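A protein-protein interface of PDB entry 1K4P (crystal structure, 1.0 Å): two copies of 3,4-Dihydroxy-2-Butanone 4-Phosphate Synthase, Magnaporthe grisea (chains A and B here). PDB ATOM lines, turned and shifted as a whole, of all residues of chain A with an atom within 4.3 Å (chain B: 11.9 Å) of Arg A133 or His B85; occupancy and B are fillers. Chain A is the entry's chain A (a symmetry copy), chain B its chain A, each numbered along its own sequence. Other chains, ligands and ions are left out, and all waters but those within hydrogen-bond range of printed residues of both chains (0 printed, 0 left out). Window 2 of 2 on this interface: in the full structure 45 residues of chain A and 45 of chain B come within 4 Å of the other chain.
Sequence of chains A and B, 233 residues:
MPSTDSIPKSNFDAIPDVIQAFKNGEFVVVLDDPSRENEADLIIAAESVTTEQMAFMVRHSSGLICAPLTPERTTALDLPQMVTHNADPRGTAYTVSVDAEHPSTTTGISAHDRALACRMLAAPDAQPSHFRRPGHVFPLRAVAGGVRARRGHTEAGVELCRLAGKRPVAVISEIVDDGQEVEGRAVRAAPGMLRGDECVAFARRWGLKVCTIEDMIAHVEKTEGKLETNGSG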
ATOM      1  N   LEU A  77     -12.907  22.266 -40.815  1.00  0.00           N
ATOM      2  CA  LEU A  77     -13.790  21.225 -40.354  1.00  0.00           C
ATOM      3  C   LEU A  77     -14.672  21.660 -39.221  1.00  0.00           C
ATOM      4  O   LEU A  77     -15.423  20.853 -38.681  1.00  0.00           O
ATOM      5  CB  LEU A  77     -12.972  19.995 -39.932  1.00  0.00           C
ATOM      6  CG  LEU A  77     -12.063  19.440 -41.057  1.00  0.00           C
ATOM      7  CD1 LEU A  77     -11.303  18.173 -40.568  1.00  0.00           C
ATOM      8  CD2 LEU A  77     -12.893  19.142 -42.294  1.00  0.00           C
ATOM      9  N   ASP A  78     -14.593  22.933 -38.860  1.00  0.00           N
ATOM     10  CA  ASP A  78     -15.457  23.496 -37.810  1.00  0.00           C
ATOM     11  C   ASP A  78     -15.362  22.756 -36.477  1.00  0.00           C
ATOM     12  O   ASP A  78     -16.352  22.214 -35.929  1.00  0.00           O
ATOM     13  CB  ASP A  78     -16.927  23.603 -38.299  1.00  0.00           C
ATOM     14  CG  ASP A  78     -17.761  24.593 -37.498  1.00  0.00           C
ATOM     15  OD1 ASP A  78     -17.316  25.298 -36.590  1.00  0.00           O
ATOM     16  OD2 ASP A  78     -19.044  24.547 -37.796  1.00  0.00           O
ATOM     17  N   LEU A  79     -14.157  22.751 -35.929  1.00  0.00           N
ATOM     18  CA  LEU A  79     -13.855  22.094 -34.672  1.00  0.00           C
ATOM     19  C   LEU A  79     -13.479  23.154 -33.652  1.00  0.00           C
ATOM     20  O   LEU A  79     -12.327  23.536 -33.499  1.00  0.00           O
ATOM     21  CB  LEU A  79     -12.674  21.102 -34.899  1.00  0.00           C
ATOM     22  CG  LEU A  79     -12.979  20.033 -35.944  1.00  0.00           C
ATOM     23  CD1 LEU A  79     -11.706  19.213 -36.205  1.00  0.00           C
ATOM     24  CD2 LEU A  79     -14.067  19.125 -35.396  1.00  0.00           C
ATOM     25  N   VAL A  96     -13.464  20.248 -29.538  1.00  0.00           N
ATOM     26  CA  VAL A  96     -14.536  19.388 -29.066  1.00  0.00           C
ATOM     27  C   VAL A  96     -14.186  17.987 -29.653  1.00  0.00           C
ATOM     28  O   VAL A  96     -13.539  17.891 -30.731  1.00  0.00           O
ATOM     29  CB  VAL A  96     -15.866  19.939 -29.634  1.00  0.00           C
ATOM     30  CG1 VAL A  96     -15.849  19.893 -31.146  1.00  0.00           C
ATOM     31  CG2 VAL A  96     -17.033  19.092 -29.194  1.00  0.00           C
ATOM     32  N   SER A  97     -14.619  16.921 -28.979  1.00  0.00           N
ATOM     33  CA  SER A  97     -14.356  15.560 -29.462  1.00  0.00           C
ATOM     34  C   SER A  97     -15.272  15.217 -30.606  1.00  0.00           C
ATOM     35  O   SER A  97     -16.337  15.857 -30.794  1.00  0.00           O
ATOM     36  CB  SER A  97     -14.506  14.577 -28.311  1.00  0.00           C
ATOM     37  OG  SER A  97     -15.810  14.734 -27.741  1.00  0.00           O
ATOM     38  N   VAL A  98     -14.869  14.172 -31.369  1.00  0.00           N
ATOM     39  CA  VAL A  98     -15.653  13.739 -32.530  1.00  0.00           C
ATOM     40  C   VAL A  98     -15.759  12.239 -32.713  1.00  0.00           C
ATOM     41  O   VAL A  98     -14.886  11.474 -32.273  1.00  0.00           O
ATOM     42  CB  VAL A  98     -15.052  14.282 -33.869  1.00  0.00           C
ATOM     43  CG1 VAL A  98     -15.012  15.821 -33.859  1.00  0.00           C
ATOM     44  CG2 VAL A  98     -13.653  13.692 -34.117  1.00  0.00           C
ATOM     45  N   PRO A 128     -17.243  19.587 -42.299  1.00  0.00           N
ATOM     46  CA  PRO A 128     -17.770  19.580 -40.947  1.00  0.00           C
ATOM     47  C   PRO A 128     -18.823  18.542 -40.676  1.00  0.00           C
ATOM     48  O   PRO A 128     -18.846  17.935 -39.591  1.00  0.00           O
ATOM     49  CB  PRO A 128     -18.273  21.005 -40.719  1.00  0.00           C
ATOM     50  CG  PRO A 128     -17.358  21.852 -41.603  1.00  0.00           C
ATOM     51  CD  PRO A 128     -17.146  20.976 -42.838  1.00  0.00           C
ATOM     52  N   PHE A 131     -18.433  14.759 -39.200  1.00  0.00           N
ATOM     53  CA  PHE A 131     -18.132  14.436 -37.793  1.00  0.00           C
ATOM     54  C   PHE A 131     -19.289  14.745 -36.864  1.00  0.00           C
ATOM     55  O   PHE A 131     -20.001  15.746 -37.043  1.00  0.00           O
ATOM     56  CB  PHE A 131     -16.905  15.238 -37.306  1.00  0.00           C
ATOM     57  CG  PHE A 131     -15.793  15.040 -38.307  1.00  0.00           C
ATOM     58  CD1 PHE A 131     -15.553  15.950 -39.340  1.00  0.00           C
ATOM     59  CD2 PHE A 131     -15.046  13.860 -38.285  1.00  0.00           C
ATOM     60  CE1 PHE A 131     -14.567  15.764 -40.313  1.00  0.00           C
ATOM     61  CE2 PHE A 131     -14.101  13.609 -39.274  1.00  0.00           C
ATOM     62  CZ  PHE A 131     -13.860  14.556 -40.276  1.00  0.00           C
ATOM     63  N   ARG A 132     -19.477  13.867 -35.872  1.00  0.00           N
ATOM     64  CA  ARG A 132     -20.505  14.057 -34.850  1.00  0.00           C
ATOM     65  C   ARG A 132     -19.770  14.637 -33.665  1.00  0.00           C
ATOM     66  O   ARG A 132     -18.671  14.150 -33.368  1.00  0.00           O
ATOM     67  CB  ARG A 132     -21.019  12.701 -34.391  1.00  0.00           C
ATOM     68  CG  ARG A 132     -21.801  11.975 -35.471  1.00  0.00           C
ATOM     69  CD  ARG A 132     -22.214  10.576 -35.025  1.00  0.00           C
ATOM     70  NE  ARG A 132     -22.681   9.801 -36.158  1.00  0.00           N
ATOM     71  CZ  ARG A 132     -22.859   8.485 -36.116  1.00  0.00           C
ATOM     72  NH1 ARG A 132     -22.618   7.824 -35.005  1.00  0.00           N
ATOM     73  NH2 ARG A 132     -23.294   7.814 -37.186  1.00  0.00           N
ATOM     74  N   ARG A 133     -20.313  15.630 -32.960  1.00  0.00           N
ATOM     75  CA  ARG A 133     -19.687  16.193 -31.776  1.00  0.00           C
ATOM     76  C   ARG A 133     -20.734  16.120 -30.669  1.00  0.00           C
ATOM     77  O   ARG A 133     -21.906  16.437 -30.917  1.00  0.00           O
ATOM     78  CB  ARG A 133     -19.271  17.649 -31.997  1.00  0.00           C
ATOM     79  CG  ARG A 133     -18.582  17.914 -33.380  1.00  0.00           C
ATOM     80  CD  ARG A 133     -19.654  18.147 -34.549  1.00  0.00           C
ATOM     81  NE  ARG A 133     -19.139  18.284 -35.948  1.00  0.00           N
ATOM     82  CZ  ARG A 133     -18.205  19.206 -36.151  1.00  0.00           C
ATOM     83  NH1 ARG A 133     -17.860  19.999 -35.132  1.00  0.00           N
ATOM     84  NH2 ARG A 133     -17.612  19.331 -37.355  1.00  0.00           N
ATOM     85  N   PRO A 134     -20.387  15.681 -29.466  1.00  0.00           N
ATOM     86  CA  PRO A 134     -19.067  15.218 -29.054  1.00  0.00           C
ATOM     87  C   PRO A 134     -18.910  13.755 -29.483  1.00  0.00           C
ATOM     88  O   PRO A 134     -19.789  13.129 -30.104  1.00  0.00           O
ATOM     89  CB  PRO A 134     -19.126  15.320 -27.518  1.00  0.00           C
ATOM     90  CG  PRO A 134     -20.595  15.020 -27.211  1.00  0.00           C
ATOM     91  CD  PRO A 134     -21.391  15.620 -28.351  1.00  0.00           C
ATOM     92  N   PRO B  80     -19.297  22.573 -16.682  1.00  0.00           N
ATOM     93  CA  PRO B  80     -20.240  22.804 -17.771  1.00  0.00           C
ATOM     94  C   PRO B  80     -20.256  21.664 -18.812  1.00  0.00           C
ATOM     95  O   PRO B  80     -19.272  20.894 -18.961  1.00  0.00           O
ATOM     96  CB  PRO B  80     -19.658  24.074 -18.451  1.00  0.00           C
ATOM     97  CG  PRO B  80     -18.206  24.203 -18.019  1.00  0.00           C
ATOM     98  CD  PRO B  80     -18.156  23.539 -16.642  1.00  0.00           C
ATOM     99  N   GLN B  81     -21.340  21.502 -19.547  1.00  0.00           N
ATOM    100  CA  GLN B  81     -21.380  20.492 -20.575  1.00  0.00           C
ATOM    101  C   GLN B  81     -20.369  20.877 -21.659  1.00  0.00           C
ATOM    102  O   GLN B  81     -20.126  22.074 -21.940  1.00  0.00           O
ATOM    103  CB  GLN B  81     -22.757  20.393 -21.243  1.00  0.00           C
ATOM    104  CG  GLN B  81     -23.782  19.674 -20.355  1.00  0.00           C
ATOM    105  CD  GLN B  81     -23.418  18.206 -20.151  1.00  0.00           C
ATOM    106  OE1 GLN B  81     -22.981  17.786 -19.030  1.00  0.00           O
ATOM    107  NE2 GLN B  81     -23.509  17.424 -21.197  1.00  0.00           N
ATOM    108  N   MET B  82     -19.750  19.853 -22.288  1.00  0.00           N
ATOM    109  CA  MET B  82     -18.771  20.096 -23.316  1.00  0.00           C
ATOM    110  C   MET B  82     -19.367  20.789 -24.524  1.00  0.00           C
ATOM    111  O   MET B  82     -18.690  21.634 -25.119  1.00  0.00           O
ATOM    112  CB  MET B  82     -18.190  18.731 -23.749  1.00  0.00           C
ATOM    113  CG  MET B  82     -16.928  18.941 -24.585  1.00  0.00           C
ATOM    114  SD  MET B  82     -16.354  17.353 -25.294  1.00  0.00           S
ATOM    115  CE  MET B  82     -15.574  16.583 -23.859  1.00  0.00           C
ATOM    116  N   VAL B  83     -20.560  20.407 -24.923  1.00  0.00           N
ATOM    117  CA  VAL B  83     -21.177  21.034 -26.084  1.00  0.00           C
ATOM    118  C   VAL B  83     -22.568  21.520 -25.747  1.00  0.00           C
ATOM    119  O   VAL B  83     -23.237  20.902 -24.936  1.00  0.00           O
ATOM    120  CB  VAL B  83     -21.380  20.062 -27.248  1.00  0.00           C
ATOM    121  CG1 VAL B  83     -20.113  19.282 -27.581  1.00  0.00           C
ATOM    122  CG2 VAL B  83     -22.547  19.118 -26.977  1.00  0.00           C
ATOM    123  N   THR B  84     -23.015  22.582 -26.423  1.00  0.00           N
ATOM    124  CA  THR B  84     -24.379  23.064 -26.243  1.00  0.00           C
ATOM    125  C   THR B  84     -25.311  22.298 -27.175  1.00  0.00           C
ATOM    126  O   THR B  84     -26.497  22.130 -26.882  1.00  0.00           O
ATOM    127  CB  THR B  84     -24.482  24.553 -26.592  1.00  0.00           C
ATOM    128  OG1 THR B  84     -24.010  24.700 -27.910  1.00  0.00           O
ATOM    129  CG2 THR B  84     -23.618  25.345 -25.625  1.00  0.00           C
ATOM    130  N   HIS B  85     -24.776  21.853 -28.331  1.00  0.00           N
ATOM    131  CA  HIS B  85     -25.563  21.117 -29.336  1.00  0.00           C
ATOM    132  C   HIS B  85     -24.992  19.719 -29.436  1.00  0.00           C
ATOM    133  O   HIS B  85     -24.200  19.419 -30.335  1.00  0.00           O
ATOM    134  CB  HIS B  85     -25.743  21.841 -30.706  1.00  0.00           C
ATOM    135  CG  HIS B  85     -26.256  23.250 -30.523  1.00  0.00           C
ATOM    136  ND1 HIS B  85     -27.604  23.585 -30.598  1.00  0.00           N
ATOM    137  CD2 HIS B  85     -25.628  24.392 -30.114  1.00  0.00           C
ATOM    138  CE1 HIS B  85     -27.760  24.888 -30.234  1.00  0.00           C
ATOM    139  NE2 HIS B  85     -26.563  25.388 -29.964  1.00  0.00           N
ATOM    140  N   ASN B  86     -25.412  18.904 -28.467  1.00  0.00           N
ATOM    141  CA  ASN B  86     -24.971  17.520 -28.324  1.00  0.00           C
ATOM    142  C   ASN B  86     -25.442  16.674 -29.533  1.00  0.00           C
ATOM    143  O   ASN B  86     -26.620  16.421 -29.740  1.00  0.00           O
ATOM    144  CB  ASN B  86     -25.498  17.052 -26.945  1.00  0.00           C
ATOM    145  CG  ASN B  86     -24.582  16.700 -25.746  1.00  0.00           C
ATOM    146  OD1 ASN B  86     -23.986  15.604 -25.741  1.00  0.00           O
ATOM    147  ND2 ASN B  86     -24.643  17.459 -24.610  1.00  0.00           N
ATOM    148  N   ALA B  87     -24.500  16.224 -30.370  1.00  0.00           N
ATOM    149  CA  ALA B  87     -24.811  15.429 -31.548  1.00  0.00           C
ATOM    150  C   ALA B  87     -24.544  13.928 -31.390  1.00  0.00           C
ATOM    151  O   ALA B  87     -24.564  13.161 -32.369  1.00  0.00           O
ATOM    152  CB  ALA B  87     -24.037  15.990 -32.734  1.00  0.00           C
ATOM    153  N   ASP B  88     -24.288  13.473 -30.150  1.00  0.00           N
ATOM    154  CA  ASP B  88     -24.089  12.034 -29.880  1.00  0.00           C
ATOM    155  C   ASP B  88     -25.475  11.357 -29.963  1.00  0.00           C
ATOM    156  O   ASP B  88     -26.466  11.957 -29.495  1.00  0.00           O
ATOM    157  CB  ASP B  88     -23.475  11.866 -28.488  1.00  0.00           C
ATOM    158  CG  ASP B  88     -23.295  10.429 -28.036  1.00  0.00           C
ATOM    159  OD1 ASP B  88     -24.182   9.798 -27.483  1.00  0.00           O
ATOM    160  OD2 ASP B  88     -22.057   9.996 -28.159  1.00  0.00           O
ATOM    161  N   PRO B  89     -25.620  10.181 -30.610  1.00  0.00           N
ATOM    162  CA  PRO B  89     -26.956   9.580 -30.762  1.00  0.00           C
ATOM    163  C   PRO B  89     -27.675   9.274 -29.455  1.00  0.00           C
ATOM    164  O   PRO B  89     -28.918   9.328 -29.365  1.00  0.00           O
ATOM    165  CB  PRO B  89     -26.798   8.310 -31.613  1.00  0.00           C
ATOM    166  CG  PRO B  89     -25.339   8.219 -32.039  1.00  0.00           C
ATOM    167  CD  PRO B  89     -24.600   9.368 -31.355  1.00  0.00           C
ATOM    168  N   ARG B  90     -26.838   8.967 -28.457  1.00  0.00           N
ATOM    169  CA  ARG B  90     -27.316   8.645 -27.120  1.00  0.00           C
ATOM    170  C   ARG B  90     -27.362   9.809 -26.109  1.00  0.00           C
ATOM    171  O   ARG B  90     -27.810   9.725 -24.956  1.00  0.00           O
ATOM    172  CB  ARG B  90     -26.681   7.352 -26.644  1.00  0.00           C
ATOM    173  CG  ARG B  90     -27.039   6.275 -27.656  1.00  0.00           C
ATOM    174  CD  ARG B  90     -26.798   4.855 -27.183  1.00  0.00           C
ATOM    175  NE  ARG B  90     -27.350   3.902 -28.136  1.00  0.00           N
ATOM    176  CZ  ARG B  90     -26.665   3.324 -29.129  1.00  0.00           C
ATOM    177  NH1 ARG B  90     -25.366   3.560 -29.357  1.00  0.00           N
ATOM    178  NH2 ARG B  90     -27.305   2.474 -29.938  1.00  0.00           N
ATOM    179  N   GLY B  91     -26.916  10.953 -26.560  1.00  0.00           N
ATOM    180  CA  GLY B  91     -26.930  12.115 -25.732  1.00  0.00           C
ATOM    181  C   GLY B  91     -25.935  11.988 -24.594  1.00  0.00           C
ATOM    182  O   GLY B  91     -26.190  12.602 -23.594  1.00  0.00           O
ATOM    183  N   THR B  92     -24.853  11.230 -24.759  1.00  0.00           N
ATOM    184  CA  THR B  92     -23.858  11.100 -23.669  1.00  0.00           C
ATOM    185  C   THR B  92     -23.461  12.483 -23.189  1.00  0.00           C
ATOM    186  O   THR B  92     -22.971  13.312 -23.954  1.00  0.00           O
ATOM    187  CB  THR B  92     -22.620  10.335 -24.159  1.00  0.00           C
ATOM    188  OG1 THR B  92     -23.115   9.122 -24.714  1.00  0.00           O
ATOM    189  CG2 THR B  92     -21.641  10.148 -22.994  1.00  0.00           C
ATOM    190  N   ALA B  93     -23.691  12.728 -21.902  1.00  0.00           N
ATOM    191  CA  ALA B  93     -23.532  14.047 -21.360  1.00  0.00           C
ATOM    192  C   ALA B  93     -22.190  14.429 -20.826  1.00  0.00           C
ATOM    193  O   ALA B  93     -22.014  14.686 -19.633  1.00  0.00           O
ATOM    194  CB  ALA B  93     -24.671  14.255 -20.360  1.00  0.00           C
ATOM    195  N   TYR B  94     -21.209  14.537 -21.722  1.00  0.00           N
ATOM    196  CA  TYR B  94     -19.876  14.883 -21.285  1.00  0.00           C
ATOM    197  C   TYR B  94     -19.772  16.289 -20.760  1.00  0.00           C
ATOM    198  O   TYR B  94     -20.290  17.224 -21.417  1.00  0.00           O
ATOM    199  CB  TYR B  94     -18.892  14.899 -22.465  1.00  0.00           C
ATOM    200  CG  TYR B  94     -18.774  13.579 -23.155  1.00  0.00           C
ATOM    201  CD1 TYR B  94     -19.508  13.294 -24.304  1.00  0.00           C
ATOM    202  CD2 TYR B  94     -17.896  12.624 -22.644  1.00  0.00           C
ATOM    203  CE1 TYR B  94     -19.371  12.058 -24.926  1.00  0.00           C
ATOM    204  CE2 TYR B  94     -17.750  11.385 -23.266  1.00  0.00           C
ATOM    205  CZ  TYR B  94     -18.490  11.109 -24.412  1.00  0.00           C
ATOM    206  OH  TYR B  94     -18.332   9.883 -25.006  1.00  0.00           O
ATOM    207  N   THR B  95     -19.095  16.466 -19.625  1.00  0.00           N
ATOM    208  CA  THR B  95     -18.818  17.824 -19.175  1.00  0.00           C
ATOM    209  C   THR B  95     -17.436  18.151 -19.787  1.00  0.00           C
ATOM    210  O   THR B  95     -16.799  17.320 -20.471  1.00  0.00           O
ATOM    211  CB  THR B  95     -18.683  17.906 -17.636  1.00  0.00           C
ATOM    212  OG1 THR B  95     -17.509  17.239 -17.140  1.00  0.00           O
ATOM    213  CG2 THR B  95     -19.931  17.350 -16.934  1.00  0.00           C
ATOM    214  N   LEU B 140     -19.326  12.669 -16.612  1.00  0.00           N
ATOM    215  CA  LEU B 140     -20.533  12.494 -17.382  1.00  0.00           C
ATOM    216  C   LEU B 140     -21.720  12.784 -16.478  1.00  0.00           C
ATOM    217  O   LEU B 140     -21.841  12.214 -15.400  1.00  0.00           O
ATOM    218  CB  LEU B 140     -20.708  11.058 -17.877  1.00  0.00           C
ATOM    219  CG  LEU B 140     -19.532  10.536 -18.715  1.00  0.00           C
ATOM    220  CD1 LEU B 140     -19.747   9.040 -19.004  1.00  0.00           C
ATOM    221  CD2 LEU B 140     -19.510  11.286 -20.053  1.00  0.00           C
ATOM    222  N   ARG B 141     -22.637  13.630 -16.929  1.00  0.00           N
ATOM    223  CA  ARG B 141     -23.819  13.985 -16.138  1.00  0.00           C
ATOM    224  C   ARG B 141     -24.940  12.973 -16.290  1.00  0.00           C
ATOM    225  O   ARG B 141     -25.579  12.899 -17.346  1.00  0.00           O
ATOM    226  CB  ARG B 141     -24.288  15.410 -16.542  1.00  0.00           C
ATOM    227  CG  ARG B 141     -25.375  15.940 -15.581  1.00  0.00           C
ATOM    228  CD  ARG B 141     -25.821  17.368 -15.986  1.00  0.00           C
ATOM    229  NE  ARG B 141     -26.381  17.354 -17.355  1.00  0.00           N
ATOM    230  CZ  ARG B 141     -26.607  18.454 -18.096  1.00  0.00           C
ATOM    231  NH1 ARG B 141     -26.380  19.678 -17.628  1.00  0.00           N
ATOM    232  NH2 ARG B 141     -27.082  18.290 -19.318  1.00  0.00           N
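Of the 18 printed residues of chain B, 7 touch a printed residue of chain A.
Of the 11 printed residues of chain A, 4 touch a printed residue of chain B.
Hydrophobic or aromatic side chains of chain A that line the printed part of chain B: Val A96 and Pro A134.
OG of Ser A97 lies within hydrogen-bond range of SD of Met B82, at 3.6 Å.
The backbone carbonyl oxygen of Arg A133 sits at hydrogen-bond distance from the backbone NH of Ala B87 (2.7 Å).
Arg A133 touches just these residues of chain B: His B85, Asn B86, Ala B87 and Asp B88.
No residue of chain B comes within 4 Å of Leu A77.
No residue of chain B comes within 4 Å of Asp A78.
No residue of chain B comes within 4 Å of Leu A79.
Val A96 touches just one residue of chain B: Val B83.
Of the printed residues of chain B, Ser A97 touches Met B82 (3.6 Å).
No residue of chain B comes within 4 Å of Pro A128.
Of chain B, only Val B83, Asn B86, Ala B87 and Tyr B94 come within 4 Å of Pro A134.
Printed residues of chain A within 4 Å of Met B82: Ser A97 (3.6 Å).
Of the printed residues of chain A, Asn B86 touches Arg A133 and Pro A134.
Printed residues of chain A within 4 Å of Val B83: Val A96 and Pro A134.
Of the printed residues of chain A, Tyr B94 touches Pro A134 (3.6 Å).
Ala B93 touches none of the printed residues of chain A.
The nearest printed residue of chain A that does not touch His B85 is Pro A134 (5.1 Å).
Val B83 touches Val A96.
O of His B85 touches O of Arg A133, at 3.8 Å.
Arg A133 touches Asn B86 (O to C, 3.8 Å).
Arg A133 touches Asp B88 (O to N, 3.9 Å).
Pro A134 touches Val B83 (CD to CG2, 3.9 Å).
Pro A134 touches Asn B86 (CD to OD1, 3.7 Å).
Pro A134 touches Ala B87.
Pro A134 touches Tyr B94 (CG to CD1, 3.6 Å).
The side-chain amide nitrogen (NE2) of Gln B81 is in hydrogen-bond range of the backbone carbonyl oxygen (O) of Tyr B94 (3.2 Å).
The backbone carbonyl oxygen (O) of Tyr B94 sits at hydrogen-bond distance from the backbone NH (N) of Met B82 (2.8 Å).
The side-chain hydroxyl (OG1) of Thr B84 sits close to a ring nitrogen (NE2) of His B85 (3.3 Å).
The side-chain carboxylate (OD1) of Asp B88 sits at hydrogen-bond distance from the side-chain hydroxyl (OG1) of Thr B92 (3.0 Å).
NH2 of Arg A133 sits at hydrogen-bond distance from O of Leu A77 (3.0 Å).
The guanidinium group (NE) of Arg A133 is in hydrogen-bond range of the backbone carbonyl oxygen (O) of Phe A131, 2.9 Å away.
No position is printed for both chains.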
